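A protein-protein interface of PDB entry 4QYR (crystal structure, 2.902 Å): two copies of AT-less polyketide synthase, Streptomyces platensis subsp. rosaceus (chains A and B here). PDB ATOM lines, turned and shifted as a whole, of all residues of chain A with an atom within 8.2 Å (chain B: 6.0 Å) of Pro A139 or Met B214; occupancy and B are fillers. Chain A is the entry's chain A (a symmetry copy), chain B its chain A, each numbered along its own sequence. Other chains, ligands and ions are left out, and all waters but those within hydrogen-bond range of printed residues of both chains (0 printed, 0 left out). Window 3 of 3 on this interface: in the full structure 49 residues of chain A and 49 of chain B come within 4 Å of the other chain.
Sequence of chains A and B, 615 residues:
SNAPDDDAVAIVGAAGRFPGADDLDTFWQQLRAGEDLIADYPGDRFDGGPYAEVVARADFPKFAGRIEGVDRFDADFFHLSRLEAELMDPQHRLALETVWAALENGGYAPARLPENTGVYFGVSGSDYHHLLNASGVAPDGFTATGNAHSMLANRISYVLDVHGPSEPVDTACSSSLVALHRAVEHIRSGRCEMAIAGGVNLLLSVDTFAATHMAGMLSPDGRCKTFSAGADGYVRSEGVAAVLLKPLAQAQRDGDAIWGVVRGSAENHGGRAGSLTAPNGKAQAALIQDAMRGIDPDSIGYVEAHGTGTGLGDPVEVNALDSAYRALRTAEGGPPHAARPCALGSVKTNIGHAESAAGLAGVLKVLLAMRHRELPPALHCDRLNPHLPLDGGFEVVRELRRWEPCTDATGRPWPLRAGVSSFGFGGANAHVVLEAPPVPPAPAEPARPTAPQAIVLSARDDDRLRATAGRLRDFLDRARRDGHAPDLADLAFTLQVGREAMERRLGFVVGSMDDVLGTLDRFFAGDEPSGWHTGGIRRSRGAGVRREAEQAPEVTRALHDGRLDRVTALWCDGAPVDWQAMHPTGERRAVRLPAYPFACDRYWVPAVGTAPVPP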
ATOM      1  N   LEU A  87      -8.276  25.746 -18.958  1.00  0.00           N
ATOM      2  CA  LEU A  87      -8.577  25.433 -20.334  1.00  0.00           C
ATOM      3  C   LEU A  87      -7.620  26.190 -21.236  1.00  0.00           C
ATOM      4  O   LEU A  87      -7.764  26.172 -22.463  1.00  0.00           O
ATOM      5  CB  LEU A  87     -10.021  25.787 -20.662  1.00  0.00           C
ATOM      6  CG  LEU A  87     -10.992  25.079 -19.727  1.00  0.00           C
ATOM      7  CD1 LEU A  87     -12.401  25.615 -19.864  1.00  0.00           C
ATOM      8  CD2 LEU A  87     -10.957  23.579 -19.992  1.00  0.00           C
ATOM      9  N   HIS A 129      -5.165  21.120 -26.624  1.00  0.00           N
ATOM     10  CA  HIS A 129      -6.551  21.103 -27.053  1.00  0.00           C
ATOM     11  C   HIS A 129      -6.926  19.690 -27.404  1.00  0.00           C
ATOM     12  O   HIS A 129      -8.055  19.266 -27.162  1.00  0.00           O
ATOM     13  CB  HIS A 129      -6.753  22.028 -28.241  1.00  0.00           C
ATOM     14  CG  HIS A 129      -8.177  22.408 -28.491  1.00  0.00           C
ATOM     15  ND1 HIS A 129      -9.244  21.723 -27.947  1.00  0.00           N
ATOM     16  CD2 HIS A 129      -8.709  23.413 -29.228  1.00  0.00           C
ATOM     17  CE1 HIS A 129     -10.372  22.290 -28.333  1.00  0.00           C
ATOM     18  NE2 HIS A 129     -10.075  23.319 -29.110  1.00  0.00           N
ATOM     19  N   LEU A 132      -7.444  17.940 -24.037  1.00  0.00           N
ATOM     20  CA  LEU A 132      -8.750  18.253 -23.454  1.00  0.00           C
ATOM     21  C   LEU A 132      -9.824  17.364 -24.027  1.00  0.00           C
ATOM     22  O   LEU A 132     -10.682  16.840 -23.314  1.00  0.00           O
ATOM     23  CB  LEU A 132      -9.144  19.707 -23.720  1.00  0.00           C
ATOM     24  CG  LEU A 132      -8.398  20.818 -22.994  1.00  0.00           C
ATOM     25  CD1 LEU A 132      -9.081  22.131 -23.263  1.00  0.00           C
ATOM     26  CD2 LEU A 132      -8.362  20.523 -21.509  1.00  0.00           C
ATOM     27  N   ASN A 133      -9.795  17.230 -25.344  1.00  0.00           N
ATOM     28  CA  ASN A 133     -10.810  16.445 -26.013  1.00  0.00           C
ATOM     29  C   ASN A 133     -10.690  14.989 -25.625  1.00  0.00           C
ATOM     30  O   ASN A 133     -11.692  14.329 -25.349  1.00  0.00           O
ATOM     31  CB  ASN A 133     -10.703  16.626 -27.519  1.00  0.00           C
ATOM     32  CG  ASN A 133     -11.129  18.003 -27.955  1.00  0.00           C
ATOM     33  OD1 ASN A 133     -11.188  18.926 -27.147  1.00  0.00           O
ATOM     34  ND2 ASN A 133     -11.423  18.155 -29.237  1.00  0.00           N
ATOM     35  N   GLY A 136     -12.185  14.225 -22.379  1.00  0.00           N
ATOM     36  CA  GLY A 136     -13.635  14.282 -22.350  1.00  0.00           C
ATOM     37  C   GLY A 136     -14.174  15.634 -21.941  1.00  0.00           C
ATOM     38  O   GLY A 136     -15.354  15.774 -21.660  1.00  0.00           O
ATOM     39  N   VAL A 137     -13.307  16.637 -21.916  1.00  0.00           N
ATOM     40  CA  VAL A 137     -13.686  17.955 -21.438  1.00  0.00           C
ATOM     41  C   VAL A 137     -14.604  18.639 -22.425  1.00  0.00           C
ATOM     42  O   VAL A 137     -14.185  18.988 -23.537  1.00  0.00           O
ATOM     43  CB  VAL A 137     -12.445  18.824 -21.195  1.00  0.00           C
ATOM     44  CG1 VAL A 137     -12.836  20.203 -20.727  1.00  0.00           C
ATOM     45  CG2 VAL A 137     -11.550  18.157 -20.179  1.00  0.00           C
ATOM     46  N   ALA A 138     -15.860  18.826 -22.028  1.00  0.00           N
ATOM     47  CA  ALA A 138     -16.822  19.539 -22.864  1.00  0.00           C
ATOM     48  C   ALA A 138     -16.285  20.928 -23.204  1.00  0.00           C
ATOM     49  O   ALA A 138     -15.513  21.509 -22.441  1.00  0.00           O
ATOM     50  CB  ALA A 138     -18.152  19.641 -22.177  1.00  0.00           C
ATOM     51  N   PRO A 139     -16.661  21.450 -24.374  1.00  0.00           N
ATOM     52  CA  PRO A 139     -16.207  22.793 -24.750  1.00  0.00           C
ATOM     53  C   PRO A 139     -16.737  23.896 -23.830  1.00  0.00           C
ATOM     54  O   PRO A 139     -17.872  23.815 -23.351  1.00  0.00           O
ATOM     55  CB  PRO A 139     -16.756  22.961 -26.174  1.00  0.00           C
ATOM     56  CG  PRO A 139     -17.816  21.911 -26.318  1.00  0.00           C
ATOM     57  CD  PRO A 139     -17.360  20.773 -25.479  1.00  0.00           C
ATOM     58  N   ASP A 140     -15.901  24.898 -23.565  1.00  0.00           N
ATOM     59  CA  ASP A 140     -16.356  26.127 -22.925  1.00  0.00           C
ATOM     60  C   ASP A 140     -15.933  27.301 -23.789  1.00  0.00           C
ATOM     61  O   ASP A 140     -15.164  27.132 -24.723  1.00  0.00           O
ATOM     62  CB  ASP A 140     -15.795  26.279 -21.505  1.00  0.00           C
ATOM     63  CG  ASP A 140     -16.262  27.571 -20.827  1.00  0.00           C
ATOM     64  OD1 ASP A 140     -17.486  27.849 -20.834  1.00  0.00           O
ATOM     65  OD2 ASP A 140     -15.404  28.334 -20.334  1.00  0.00           O
ATOM     66  N   GLY A 141     -16.458  28.481 -23.483  1.00  0.00           N
ATOM     67  CA  GLY A 141     -16.011  29.711 -24.094  1.00  0.00           C
ATOM     68  C   GLY A 141     -14.544  29.983 -23.847  1.00  0.00           C
ATOM     69  O   GLY A 141     -13.912  30.676 -24.634  1.00  0.00           O
ATOM     70  N   PHE A 142     -13.988  29.431 -22.776  1.00  0.00           N
ATOM     71  CA  PHE A 142     -12.581  29.652 -22.475  1.00  0.00           C
ATOM     72  C   PHE A 142     -11.665  28.757 -23.291  1.00  0.00           C
ATOM     73  O   PHE A 142     -10.470  29.058 -23.440  1.00  0.00           O
ATOM     74  CB  PHE A 142     -12.293  29.432 -20.989  1.00  0.00           C
ATOM     75  CG  PHE A 142     -12.837  30.510 -20.096  1.00  0.00           C
ATOM     76  CD1 PHE A 142     -12.751  31.842 -20.467  1.00  0.00           C
ATOM     77  CD2 PHE A 142     -13.469  30.183 -18.894  1.00  0.00           C
ATOM     78  CE1 PHE A 142     -13.270  32.826 -19.646  1.00  0.00           C
ATOM     79  CE2 PHE A 142     -13.978  31.154 -18.080  1.00  0.00           C
ATOM     80  CZ  PHE A 142     -13.888  32.475 -18.452  1.00  0.00           C
ATOM     81  N   THR A 143     -12.205  27.653 -23.805  1.00  0.00           N
ATOM     82  CA  THR A 143     -11.376  26.703 -24.549  1.00  0.00           C
ATOM     83  C   THR A 143     -10.884  27.313 -25.846  1.00  0.00           C
ATOM     84  O   THR A 143      -9.694  27.256 -26.152  1.00  0.00           O
ATOM     85  CB  THR A 143     -12.106  25.417 -24.912  1.00  0.00           C
ATOM     86  OG1 THR A 143     -12.848  24.924 -23.788  1.00  0.00           O
ATOM     87  CG2 THR A 143     -11.087  24.380 -25.364  1.00  0.00           C
ATOM     88  N   ALA A 144     -11.819  27.892 -26.594  1.00  0.00           N
ATOM     89  CA  ALA A 144     -11.526  28.538 -27.870  1.00  0.00           C
ATOM     90  C   ALA A 144     -10.483  29.647 -27.710  1.00  0.00           C
ATOM     91  O   ALA A 144      -9.453  29.668 -28.388  1.00  0.00           O
ATOM     92  CB  ALA A 144     -12.794  29.095 -28.463  1.00  0.00           C
ATOM     93  N   ASP B  59     -25.102  22.654 -28.302  1.00  0.00           N
ATOM     94  CA  ASP B  59     -26.053  23.682 -27.879  1.00  0.00           C
ATOM     95  C   ASP B  59     -26.375  24.759 -28.920  1.00  0.00           C
ATOM     96  O   ASP B  59     -27.541  25.124 -29.090  1.00  0.00           O
ATOM     97  CB  ASP B  59     -25.546  24.358 -26.603  1.00  0.00           C
ATOM     98  CG  ASP B  59     -26.681  24.869 -25.718  1.00  0.00           C
ATOM     99  OD1 ASP B  59     -27.749  25.231 -26.263  1.00  0.00           O
ATOM    100  OD2 ASP B  59     -26.508  24.902 -24.476  1.00  0.00           O
ATOM    101  N   VAL B 206     -17.575  20.651 -33.950  1.00  0.00           N
ATOM    102  CA  VAL B 206     -18.469  21.285 -32.988  1.00  0.00           C
ATOM    103  C   VAL B 206     -17.777  22.286 -32.075  1.00  0.00           C
ATOM    104  O   VAL B 206     -18.362  23.306 -31.710  1.00  0.00           O
ATOM    105  CB  VAL B 206     -19.127  20.236 -32.097  1.00  0.00           C
ATOM    106  CG1 VAL B 206     -20.213  20.863 -31.280  1.00  0.00           C
ATOM    107  CG2 VAL B 206     -19.696  19.135 -32.943  1.00  0.00           C
ATOM    108  N   ASP B 207     -16.539  21.964 -31.705  1.00  0.00           N
ATOM    109  CA  ASP B 207     -15.770  22.708 -30.718  1.00  0.00           C
ATOM    110  C   ASP B 207     -15.980  24.219 -30.728  1.00  0.00           C
ATOM    111  O   ASP B 207     -16.423  24.790 -29.727  1.00  0.00           O
ATOM    112  CB  ASP B 207     -14.280  22.412 -30.901  1.00  0.00           C
ATOM    113  CG  ASP B 207     -13.936  20.957 -30.625  1.00  0.00           C
ATOM    114  OD1 ASP B 207     -13.426  20.664 -29.510  1.00  0.00           O
ATOM    115  OD2 ASP B 207     -14.172  20.114 -31.527  1.00  0.00           O
ATOM    116  N   PHE B 209     -18.093  26.022 -32.459  1.00  0.00           N
ATOM    117  CA  PHE B 209     -19.512  26.365 -32.492  1.00  0.00           C
ATOM    118  C   PHE B 209     -20.032  26.519 -31.080  1.00  0.00           C
ATOM    119  O   PHE B 209     -20.576  27.560 -30.707  1.00  0.00           O
ATOM    120  CB  PHE B 209     -20.321  25.293 -33.224  1.00  0.00           C
ATOM    121  CG  PHE B 209     -20.411  25.503 -34.701  1.00  0.00           C
ATOM    122  CD1 PHE B 209     -21.080  26.603 -35.220  1.00  0.00           C
ATOM    123  CD2 PHE B 209     -19.843  24.586 -35.585  1.00  0.00           C
ATOM    124  CE1 PHE B 209     -21.176  26.797 -36.611  1.00  0.00           C
ATOM    125  CE2 PHE B 209     -19.931  24.765 -36.980  1.00  0.00           C
ATOM    126  CZ  PHE B 209     -20.591  25.873 -37.495  1.00  0.00           C
ATOM    127  N   ALA B 210     -19.851  25.457 -30.305  1.00  0.00           N
ATOM    128  CA  ALA B 210     -20.296  25.403 -28.926  1.00  0.00           C
ATOM    129  C   ALA B 210     -19.709  26.543 -28.127  1.00  0.00           C
ATOM    130  O   ALA B 210     -20.410  27.214 -27.380  1.00  0.00           O
ATOM    131  CB  ALA B 210     -19.913  24.069 -28.303  1.00  0.00           C
ATOM    132  N   ALA B 211     -18.417  26.768 -28.297  1.00  0.00           N
ATOM    133  CA  ALA B 211     -17.714  27.732 -27.460  1.00  0.00           C
ATOM    134  C   ALA B 211     -18.201  29.149 -27.717  1.00  0.00           C
ATOM    135  O   ALA B 211     -18.539  29.880 -26.776  1.00  0.00           O
ATOM    136  CB  ALA B 211     -16.222  27.632 -27.682  1.00  0.00           C
ATOM    137  N   THR B 212     -18.246  29.522 -28.992  1.00  0.00           N
ATOM    138  CA  THR B 212     -18.747  30.824 -29.393  1.00  0.00           C
ATOM    139  C   THR B 212     -20.136  31.074 -28.843  1.00  0.00           C
ATOM    140  O   THR B 212     -20.444  32.181 -28.409  1.00  0.00           O
ATOM    141  CB  THR B 212     -18.783  30.958 -30.908  1.00  0.00           C
ATOM    142  OG1 THR B 212     -17.544  30.483 -31.435  1.00  0.00           O
ATOM    143  CG2 THR B 212     -18.969  32.409 -31.314  1.00  0.00           C
ATOM    144  N   HIS B 213     -20.965  30.040 -28.844  1.00  0.00           N
ATOM    145  CA  HIS B 213     -22.320  30.159 -28.327  1.00  0.00           C
ATOM    146  C   HIS B 213     -22.334  30.524 -26.846  1.00  0.00           C
ATOM    147  O   HIS B 213     -23.113  31.371 -26.418  1.00  0.00           O
ATOM    148  CB  HIS B 213     -23.089  28.857 -28.551  1.00  0.00           C
ATOM    149  CG  HIS B 213     -24.512  28.916 -28.092  1.00  0.00           C
ATOM    150  ND1 HIS B 213     -25.341  29.977 -28.382  1.00  0.00           N
ATOM    151  CD2 HIS B 213     -25.249  28.048 -27.364  1.00  0.00           C
ATOM    152  CE1 HIS B 213     -26.529  29.763 -27.848  1.00  0.00           C
ATOM    153  NE2 HIS B 213     -26.499  28.600 -27.224  1.00  0.00           N
ATOM    154  N   MET B 214     -21.471  29.876 -26.071  1.00  0.00           N
ATOM    155  CA  MET B 214     -21.352  30.161 -24.642  1.00  0.00           C
ATOM    156  C   MET B 214     -20.913  31.592 -24.428  1.00  0.00           C
ATOM    157  O   MET B 214     -21.450  32.293 -23.574  1.00  0.00           O
ATOM    158  CB  MET B 214     -20.372  29.205 -23.978  1.00  0.00           C
ATOM    159  CG  MET B 214     -20.894  27.801 -23.882  1.00  0.00           C
ATOM    160  SD  MET B 214     -19.909  26.709 -22.623  1.00  0.00           S
ATOM    161  CE  MET B 214     -20.773  25.005 -23.025  1.00  0.00           C
ATOM    162  N   ALA B 215     -19.953  32.024 -25.235  1.00  0.00           N
ATOM    163  CA  ALA B 215     -19.549  33.423 -25.277  1.00  0.00           C
ATOM    164  C   ALA B 215     -20.709  34.392 -25.592  1.00  0.00           C
ATOM    165  O   ALA B 215     -20.546  35.607 -25.456  1.00  0.00           O
ATOM    166  CB  ALA B 215     -18.438  33.597 -26.293  1.00  0.00           C
ATOM    167  N   GLY B 216     -21.862  33.865 -26.018  1.00  0.00           N
ATOM    168  CA  GLY B 216     -23.006  34.692 -26.362  1.00  0.00           C
ATOM    169  C   GLY B 216     -22.800  35.510 -27.629  1.00  0.00           C
ATOM    170  O   GLY B 216     -23.186  36.676 -27.701  1.00  0.00           O
ATOM    171  N   MET B 217     -22.199  34.901 -28.644  1.00  0.00           N
ATOM    172  CA  MET B 217     -21.805  35.641 -29.835  1.00  0.00           C
ATOM    173  C   MET B 217     -22.549  35.173 -31.072  1.00  0.00           C
ATOM    174  O   MET B 217     -22.527  35.834 -32.103  1.00  0.00           O
ATOM    175  CB  MET B 217     -20.291  35.517 -30.060  1.00  0.00           C
ATOM    176  CG  MET B 217     -19.422  35.989 -28.889  1.00  0.00           C
ATOM    177  SD  MET B 217     -18.672  37.753 -29.164  1.00  0.00           S
ATOM    178  CE  MET B 217     -17.725  37.918 -27.464  1.00  0.00           C
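Of the printed residues of chain B, Pro A139 touches Ala B210 and Met B214. Met B214 touches three residues of chain A. No residue of chain A comes within 4 Å of Ala B215. Printed residues of chain B within 4 Å of Asn A133: Asp B207 (3.2 Å). Of the printed residues of chain B, Gly A141 touches Ala B211 and Met B214. Of the printed residues of chain A, Asp B207 touches His A129 (3.7 Å) and Asn A133 (3.2 Å). Printed residues of chain B within 4 Å of His A129: Asp B207 (3.7 Å). Of the printed residues of chain A, Ala B210 touches Pro A139 (3.6 Å). The nearest residue of chain A that does not touch Met B214 is Ala A138 (6.0 Å). The nearest printed residue of chain A that does not touch Ala B211 is Pro A139 (4.7 Å).
No position is printed for both chains.
The backbone NH of Asp A140 is in hydrogen-bond range of the side-chain hydroxyl of Thr A143 (3.1 Å). The side-chain carboxylate (OD2) of Asp A140 is in hydrogen-bond range of the backbone NH (N) of Phe A142 (3.0 Å). O of His A129 lies close to OD1 of Asn A133 (3.2 Å).
CE1 of His A129 touches OD1 of Asp B207, 3.7 Å away. CG of Pro A139 touches CB of Ala B210, 3.6 Å away. Asp A140 touches Ala B211 (O to CB, 3.2 Å). Gly A141 touches Ala B211 (CA to O, 3.7 Å). Gly A141 touches Met B214 (N to SD, 3.97 Å). CB of Ala B211 touches CB of Ala A144 (3.8 Å).
The side-chain carboxylate of Asp B207 lies within hydrogen-bond range of the side-chain amide nitrogen of Asn A133 (3.2 Å). The backbone carbonyl oxygen of Pro A139 lies close to the side-chain sulfur of Met B214 (3.6 Å). The side-chain carboxylate (OD1) of Asp A140 sits close to the side-chain sulfur (SD) of Met B214.
Of the 13 printed residues of chain A, 6 touch a printed residue of chain B. Printed residues of chain A that touch a printed residue of chain B: His A129, Asn A133, Pro A139, Asp A140, Gly A141 and Ala A144. Hydrophobic or aromatic side chains of chain A that line the printed part of chain B: His A129, Pro A139 and Ala A144. Along chain A the printed residues that touch a printed residue of chain B span positions 129 to 144. Of the 12 printed residues of chain B, 4 touch a printed residue of chain A. Hydrophobic or aromatic side chains of chain B that line the printed part of chain A: Ala B210, Ala B211 and Met B214. Along chain B the printed residues that touch a printed residue of chain A span positions 207 to 214. Among the printed residues, 9 pairs touch across the chains. Among the printed residues, no Asp or Glu carboxylate lies within 4 Å of a Lys or Arg side-chain nitrogen of the other chain.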
